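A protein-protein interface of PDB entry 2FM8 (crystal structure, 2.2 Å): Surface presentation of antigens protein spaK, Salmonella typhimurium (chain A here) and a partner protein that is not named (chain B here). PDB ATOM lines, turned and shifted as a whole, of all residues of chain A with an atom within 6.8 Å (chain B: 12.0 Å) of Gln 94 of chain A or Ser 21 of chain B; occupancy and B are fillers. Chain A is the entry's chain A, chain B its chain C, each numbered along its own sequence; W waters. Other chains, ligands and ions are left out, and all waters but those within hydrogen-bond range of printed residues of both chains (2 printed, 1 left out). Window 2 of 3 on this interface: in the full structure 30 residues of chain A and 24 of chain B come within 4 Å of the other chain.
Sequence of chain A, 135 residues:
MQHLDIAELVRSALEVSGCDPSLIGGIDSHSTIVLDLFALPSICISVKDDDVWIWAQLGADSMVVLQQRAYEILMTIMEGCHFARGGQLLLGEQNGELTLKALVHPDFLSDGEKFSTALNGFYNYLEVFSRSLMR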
ATOM      1  N   LYS A  48      17.724 -22.133  25.802  1.00  0.00           N
ATOM      2  CA  LYS A  48      18.928 -21.536  25.309  1.00  0.00           C
ATOM      3  C   LYS A  48      19.753 -21.278  26.545  1.00  0.00           C
ATOM      4  O   LYS A  48      19.433 -20.391  27.328  1.00  0.00           O
ATOM      5  CB  LYS A  48      18.600 -20.256  24.549  1.00  0.00           C
ATOM      6  CG  LYS A  48      19.643 -19.829  23.521  1.00  0.00           C
ATOM      7  CD  LYS A  48      19.089 -18.661  22.668  1.00  0.00           C
ATOM      8  CE  LYS A  48      20.184 -17.942  21.850  1.00  0.00           C
ATOM      9  NZ  LYS A  48      20.000 -16.428  21.870  1.00  0.00           N
ATOM     10  N   TRP A  55       8.627 -17.609  21.567  1.00  0.00           N
ATOM     11  CA  TRP A  55       8.637 -16.510  20.610  1.00  0.00           C
ATOM     12  C   TRP A  55       7.851 -16.823  19.351  1.00  0.00           C
ATOM     13  O   TRP A  55       7.446 -17.954  19.127  1.00  0.00           O
ATOM     14  CB  TRP A  55      10.059 -16.090  20.275  1.00  0.00           C
ATOM     15  CG  TRP A  55      10.758 -16.894  19.229  1.00  0.00           C
ATOM     16  CD1 TRP A  55      10.852 -16.608  17.870  1.00  0.00           C
ATOM     17  CD2 TRP A  55      11.490 -18.087  19.431  1.00  0.00           C
ATOM     18  NE1 TRP A  55      11.602 -17.559  17.239  1.00  0.00           N
ATOM     19  CE2 TRP A  55      12.000 -18.488  18.166  1.00  0.00           C
ATOM     20  CE3 TRP A  55      11.775 -18.855  20.549  1.00  0.00           C
ATOM     21  CZ2 TRP A  55      12.770 -19.615  18.003  1.00  0.00           C
ATOM     22  CZ3 TRP A  55      12.532 -19.977  20.389  1.00  0.00           C
ATOM     23  CH2 TRP A  55      13.033 -20.354  19.128  1.00  0.00           C
ATOM     24  N   GLN A  57       7.659 -15.088  15.129  1.00  0.00           N
ATOM     25  CA  GLN A  57       7.770 -14.075  14.073  1.00  0.00           C
ATOM     26  C   GLN A  57       6.410 -13.526  13.710  1.00  0.00           C
ATOM     27  O   GLN A  57       5.433 -14.266  13.671  1.00  0.00           O
ATOM     28  CB  GLN A  57       8.437 -14.669  12.841  1.00  0.00           C
ATOM     29  CG  GLN A  57       9.882 -15.002  13.079  1.00  0.00           C
ATOM     30  CD  GLN A  57      10.501 -15.698  11.893  1.00  0.00           C
ATOM     31  OE1 GLN A  57       9.904 -15.737  10.809  1.00  0.00           O
ATOM     32  NE2 GLN A  57      11.713 -16.235  12.073  1.00  0.00           N
ATOM     33  N   LEU A  58       6.332 -12.224  13.445  1.00  0.00           N
ATOM     34  CA  LEU A  58       5.048 -11.577  13.332  1.00  0.00           C
ATOM     35  C   LEU A  58       4.585 -11.300  11.906  1.00  0.00           C
ATOM     36  O   LEU A  58       3.542 -10.688  11.726  1.00  0.00           O
ATOM     37  CB  LEU A  58       5.019 -10.299  14.159  1.00  0.00           C
ATOM     38  CG  LEU A  58       5.144 -10.484  15.667  1.00  0.00           C
ATOM     39  CD1 LEU A  58       5.342  -9.135  16.332  1.00  0.00           C
ATOM     40  CD2 LEU A  58       3.935 -11.209  16.247  1.00  0.00           C
ATOM     41  N   MET A  63       7.863  -5.458   9.835  1.00  0.00           N
ATOM     42  CA  MET A  63       8.838  -4.373  10.071  1.00  0.00           C
ATOM     43  C   MET A  63       8.387  -3.064   9.402  1.00  0.00           C
ATOM     44  O   MET A  63       8.527  -1.995   9.960  1.00  0.00           O
ATOM     45  CB  MET A  63      10.239  -4.761   9.626  1.00  0.00           C
ATOM     46  CG  MET A  63      10.885  -5.868  10.484  1.00  0.00           C
ATOM     47  SD  MET A  63      11.209  -5.442  12.211  1.00  0.00           S
ATOM     48  CE  MET A  63      12.414  -4.123  12.088  1.00  0.00           C
ATOM     49  N   GLY A  92      12.392  -8.578  18.896  1.00  0.00           N
ATOM     50  CA  GLY A  92      13.577  -8.694  18.067  1.00  0.00           C
ATOM     51  C   GLY A  92      13.175  -8.796  16.599  1.00  0.00           C
ATOM     52  O   GLY A  92      12.085  -8.395  16.202  1.00  0.00           O
ATOM     53  N   GLU A  93      14.087  -9.312  15.798  1.00  0.00           N
ATOM     54  CA  GLU A  93      13.881  -9.443  14.376  1.00  0.00           C
ATOM     55  C   GLU A  93      14.565 -10.718  13.843  1.00  0.00           C
ATOM     56  O   GLU A  93      15.739 -10.915  14.037  1.00  0.00           O
ATOM     57  CB  GLU A  93      14.421  -8.212  13.639  1.00  0.00           C
ATOM     58  CG  GLU A  93      14.088  -8.298  12.143  1.00  0.00           C
ATOM     59  CD  GLU A  93      14.629  -7.197  11.304  1.00  0.00           C
ATOM     60  OE1 GLU A  93      15.381  -6.357  11.819  1.00  0.00           O
ATOM     61  OE2 GLU A  93      14.295  -7.188  10.101  1.00  0.00           O
ATOM     62  N   GLN A  94      13.812 -11.565  13.164  1.00  0.00           N
ATOM     63  CA  GLN A  94      14.328 -12.810  12.637  1.00  0.00           C
ATOM     64  C   GLN A  94      13.792 -12.964  11.236  1.00  0.00           C
ATOM     65  O   GLN A  94      12.610 -12.747  10.996  1.00  0.00           O
ATOM     66  CB  GLN A  94      13.866 -14.023  13.469  1.00  0.00           C
ATOM     67  CG  GLN A  94      14.721 -14.340  14.661  1.00  0.00           C
ATOM     68  CD  GLN A  94      16.027 -14.976  14.259  1.00  0.00           C
ATOM     69  OE1 GLN A  94      16.060 -16.090  13.714  1.00  0.00           O
ATOM     70  NE2 GLN A  94      17.116 -14.265  14.501  1.00  0.00           N
ATOM     71  N   ASN A  95      14.680 -13.369  10.329  1.00  0.00           N
ATOM     72  CA  ASN A  95      14.367 -13.511   8.924  1.00  0.00           C
ATOM     73  C   ASN A  95      13.622 -12.317   8.324  1.00  0.00           C
ATOM     74  O   ASN A  95      12.676 -12.491   7.544  1.00  0.00           O
ATOM     75  CB  ASN A  95      13.604 -14.802   8.723  1.00  0.00           C
ATOM     76  CG  ASN A  95      14.380 -15.999   9.220  1.00  0.00           C
ATOM     77  OD1 ASN A  95      15.600 -16.119   8.975  1.00  0.00           O
ATOM     78  ND2 ASN A  95      13.691 -16.883   9.952  1.00  0.00           N
ATOM     79  N   GLY A  96      14.078 -11.111   8.680  1.00  0.00           N
ATOM     80  CA  GLY A  96      13.453  -9.860   8.205  1.00  0.00           C
ATOM     81  C   GLY A  96      12.066  -9.589   8.769  1.00  0.00           C
ATOM     82  O   GLY A  96      11.316  -8.779   8.237  1.00  0.00           O
ATOM     83  N   GLU A  97      11.716 -10.271   9.861  1.00  0.00           N
ATOM     84  CA  GLU A  97      10.399 -10.141  10.463  1.00  0.00           C
ATOM     85  C   GLU A  97      10.519  -9.740  11.922  1.00  0.00           C
ATOM     86  O   GLU A  97      11.414 -10.199  12.608  1.00  0.00           O
ATOM     87  CB  GLU A  97       9.646 -11.458  10.359  1.00  0.00           C
ATOM     88  CG  GLU A  97       9.524 -12.003   8.939  1.00  0.00           C
ATOM     89  CD  GLU A  97       8.363 -13.025   8.757  1.00  0.00           C
ATOM     90  OE1 GLU A  97       7.538 -13.250   9.702  1.00  0.00           O
ATOM     91  OE2 GLU A  97       8.278 -13.559   7.628  1.00  0.00           O
ATOM     92  N   LEU A  98       9.627  -8.867  12.388  1.00  0.00           N
ATOM     93  CA  LEU A  98       9.571  -8.556  13.793  1.00  0.00           C
ATOM     94  C   LEU A  98       9.225  -9.808  14.616  1.00  0.00           C
ATOM     95  O   LEU A  98       8.335 -10.592  14.241  1.00  0.00           O
ATOM     96  CB  LEU A  98       8.535  -7.484  14.061  1.00  0.00           C
ATOM     97  CG  LEU A  98       8.564  -6.881  15.468  1.00  0.00           C
ATOM     98  CD1 LEU A  98       9.829  -6.061  15.699  1.00  0.00           C
ATOM     99  CD2 LEU A  98       7.328  -5.980  15.590  1.00  0.00           C
ATOM    100  N   THR A  99       9.898  -9.963  15.749  1.00  0.00           N
ATOM    101  CA  THR A  99       9.715 -11.120  16.616  1.00  0.00           C
ATOM    102  C   THR A  99       9.229 -10.704  18.007  1.00  0.00           C
ATOM    103  O   THR A  99       9.725  -9.745  18.604  1.00  0.00           O
ATOM    104  CB  THR A  99      11.032 -11.917  16.658  1.00  0.00           C
ATOM    105  OG1 THR A  99      11.291 -12.420  15.329  1.00  0.00           O
ATOM    106  CG2 THR A  99      10.917 -13.112  17.545  1.00  0.00           C
ATOM    107  N   LYS A 101       8.908 -11.968  21.852  1.00  0.00           N
ATOM    108  CA  LYS A 101       9.698 -12.944  22.625  1.00  0.00           C
ATOM    109  C   LYS A 101       9.393 -12.794  24.107  1.00  0.00           C
ATOM    110  O   LYS A 101       9.313 -11.669  24.618  1.00  0.00           O
ATOM    111  CB  LYS A 101      11.214 -12.703  22.482  1.00  0.00           C
ATOM    112  CG  LYS A 101      11.745 -12.526  21.099  1.00  0.00           C
ATOM    113  CD  LYS A 101      13.303 -12.512  21.094  1.00  0.00           C
ATOM    114  CE  LYS A 101      13.944 -11.269  21.684  1.00  0.00           C
ATOM    115  NZ  LYS A 101      15.521 -11.272  21.613  1.00  0.00           N
ATOM    116  N   SER B  15      11.718 -28.365  15.105  1.00  0.00           N
ATOM    117  CA  SER B  15      12.425 -27.760  14.014  1.00  0.00           C
ATOM    118  C   SER B  15      13.878 -27.582  14.404  1.00  0.00           C
ATOM    119  O   SER B  15      14.190 -27.033  15.467  1.00  0.00           O
ATOM    120  CB  SER B  15      11.793 -26.406  13.676  1.00  0.00           C
ATOM    121  OG  SER B  15      12.702 -25.581  12.984  1.00  0.00           O
ATOM    122  N   ALA B  16      14.759 -28.068  13.533  1.00  0.00           N
ATOM    123  CA  ALA B  16      16.194 -27.812  13.661  1.00  0.00           C
ATOM    124  C   ALA B  16      16.581 -26.465  13.034  1.00  0.00           C
ATOM    125  O   ALA B  16      17.657 -25.953  13.292  1.00  0.00           O
ATOM    126  CB  ALA B  16      16.989 -28.948  13.028  1.00  0.00           C
ATOM    127  N   THR B  17      15.687 -25.892  12.238  1.00  0.00           N
ATOM    128  CA  THR B  17      15.911 -24.597  11.592  1.00  0.00           C
ATOM    129  C   THR B  17      15.492 -23.402  12.491  1.00  0.00           C
ATOM    130  O   THR B  17      16.230 -22.424  12.605  1.00  0.00           O
ATOM    131  CB  THR B  17      15.198 -24.503  10.183  1.00  0.00           C
ATOM    132  OG1 THR B  17      14.662 -23.191   9.977  1.00  0.00           O
ATOM    133  CG2 THR B  17      14.047 -25.450  10.043  1.00  0.00           C
ATOM    134  N   ALA B  18      14.308 -23.487  13.105  1.00  0.00           N
ATOM    135  CA  ALA B  18      13.767 -22.400  13.920  1.00  0.00           C
ATOM    136  C   ALA B  18      14.681 -22.091  15.087  1.00  0.00           C
ATOM    137  O   ALA B  18      14.910 -22.932  15.939  1.00  0.00           O
ATOM    138  CB  ALA B  18      12.391 -22.759  14.430  1.00  0.00           C
ATOM    139  N   THR B  19      15.193 -20.876  15.131  1.00  0.00           N
ATOM    140  CA  THR B  19      16.253 -20.549  16.059  1.00  0.00           C
ATOM    141  C   THR B  19      16.219 -19.045  16.369  1.00  0.00           C
ATOM    142  O   THR B  19      15.804 -18.264  15.530  1.00  0.00           O
ATOM    143  CB  THR B  19      17.610 -21.033  15.451  1.00  0.00           C
ATOM    144  OG1 THR B  19      18.546 -21.309  16.493  1.00  0.00           O
ATOM    145  CG2 THR B  19      18.209 -20.021  14.473  1.00  0.00           C
ATOM    146  N   LEU B  20      16.606 -18.668  17.591  1.00  0.00           N
ATOM    147  CA  LEU B  20      16.732 -17.264  18.022  1.00  0.00           C
ATOM    148  C   LEU B  20      18.132 -16.681  17.720  1.00  0.00           C
ATOM    149  O   LEU B  20      19.000 -17.389  17.208  1.00  0.00           O
ATOM    150  CB  LEU B  20      16.416 -17.144  19.520  1.00  0.00           C
ATOM    151  CG  LEU B  20      14.964 -16.884  19.939  1.00  0.00           C
ATOM    152  CD1 LEU B  20      14.893 -16.667  21.429  1.00  0.00           C
ATOM    153  CD2 LEU B  20      14.365 -15.692  19.198  1.00  0.00           C
ATOM    154  N   SER B  21      18.359 -15.397  18.020  1.00  0.00           N
ATOM    155  CA  SER B  21      19.638 -14.745  17.646  1.00  0.00           C
ATOM    156  C   SER B  21      20.258 -13.779  18.676  1.00  0.00           C
ATOM    157  O   SER B  21      19.560 -12.949  19.283  1.00  0.00           O
ATOM    158  CB  SER B  21      19.472 -13.998  16.316  1.00  0.00           C
ATOM    159  OG  SER B  21      18.552 -12.914  16.436  1.00  0.00           O
ATOM    160  N   GLY B  22      21.586 -13.866  18.822  1.00  0.00           N
ATOM    161  CA  GLY B  22      22.347 -12.994  19.728  1.00  0.00           C
ATOM    162  C   GLY B  22      23.034 -11.843  19.005  1.00  0.00           C
ATOM    163  O   GLY B  22      22.373 -10.931  18.497  1.00  0.00           O
ATOM    164  N   GLU B  52      14.106  -0.301   6.251  1.00  0.00           N
ATOM    165  CA  GLU B  52      15.287  -1.178   6.206  1.00  0.00           C
ATOM    166  C   GLU B  52      16.009  -1.057   4.865  1.00  0.00           C
ATOM    167  O   GLU B  52      17.240  -1.030   4.808  1.00  0.00           O
ATOM    168  CB  GLU B  52      14.911  -2.639   6.462  1.00  0.00           C
ATOM    169  CG  GLU B  52      14.486  -2.950   7.907  1.00  0.00           C
ATOM    170  CD  GLU B  52      14.230  -4.463   8.153  1.00  0.00           C
ATOM    171  OE1 GLU B  52      13.313  -5.079   7.527  1.00  0.00           O
ATOM    172  OE2 GLU B  52      14.978  -5.043   8.974  1.00  0.00           O
HETATM  173  O   HOH W   1      18.077 -10.410  15.225  1.00  0.00           O
HETATM  174  O   HOH W   2      15.867 -18.752  12.687  1.00  0.00           O
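The side-chain carboxylate (OE2) of Glu 93 of chain A lies close to the side-chain carboxylate (OE2) of Glu 52 of chain B (2.5 Å).
The backbone carbonyl oxygen of Thr 19 of chain B lies close to the side-chain amide oxygen of Gln 94 of chain A, 2.8 Å away.
The side-chain amide nitrogen of Gln 94 of chain A is in hydrogen-bond range of the side-chain hydroxyl of Ser 21 of chain B, at 2.8 Å.
The backbone NH (N) of Leu 98 of chain A sits close to the side-chain sulfur (SD) of Met 63 of chain A, at 3.8 Å.
OG1 of Thr 99 of chain A lies within hydrogen-bond range of N of Gln 94 of chain A (3.4 Å).
Among the printed residues, pairs that only touch across the chains: Trp 55 of chain A with Thr 19 of chain B (3.9 Å), Trp 55 of chain A with Leu 20 of chain B (3.7 Å), Met 63 of chain A with Glu 52 of chain B (3.7 Å) and Lys 101 of chain A with Leu 20 of chain B (3.9 Å).
Of the printed residues of chain B, Trp 55 of chain A touches Thr 19 (3.9 Å) and Leu 20 (3.7 Å).
No residue of chain B comes within 4 Å of Gln 57 of chain A.
Of the printed residues of chain B, Met 63 of chain A touches Glu 52.
No residue of chain B comes within 4 Å of Gly 92 of chain A.
Of chain B, only Thr 19 and Ser 21 come within 4 Å of Gln 94 of chain A.
No residue of chain B comes within 4 Å of Gly 96 of chain A.
No residue of chain B comes within 4 Å of Glu 97 of chain A.
No residue of chain B comes within 4 Å of Thr 99 of chain A.
Of the printed residues of chain B, Lys 101 of chain A touches Leu 20.
Thr 17 of chain B touches none of the printed residues of chain A.
Of chain A, only Gln 94 comes within 4 Å of Ser 21 of chain B.
Printed residues of chain A within 4 Å of Glu 52 of chain B: Met 63 and Glu 93.
The nearest residue of chain B that does not touch Gln 94 of chain A is Leu 20 of chain B (4.2 Å).
The nearest residue of chain A that does not touch Ser 21 of chain B is Lys 48 of chain A (4.2 Å).
Of the 14 printed residues of chain A, 5 touch a printed residue of chain B.
Hydrophobic or aromatic side chains of chain A within 4 Å of the printed part of chain B: Trp 55 and Met 63.
Hydrophobic or aromatic side chains of chain B that line the printed part of chain A: Leu 20.
Among the printed residues, no Asp or Glu carboxylate lies within 4 Å of a Lys or Arg side-chain nitrogen of the other chain.
Water W1 bridges the backbone carbonyl oxygen (O) of Glu 93 of chain A and the side-chain hydroxyl (OG) of Ser 21 of chain B.
Water W2 bridges OE1 of Gln 94 of chain A (2.9 Å) and O of Thr 19 of chain B (2.9 Å).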
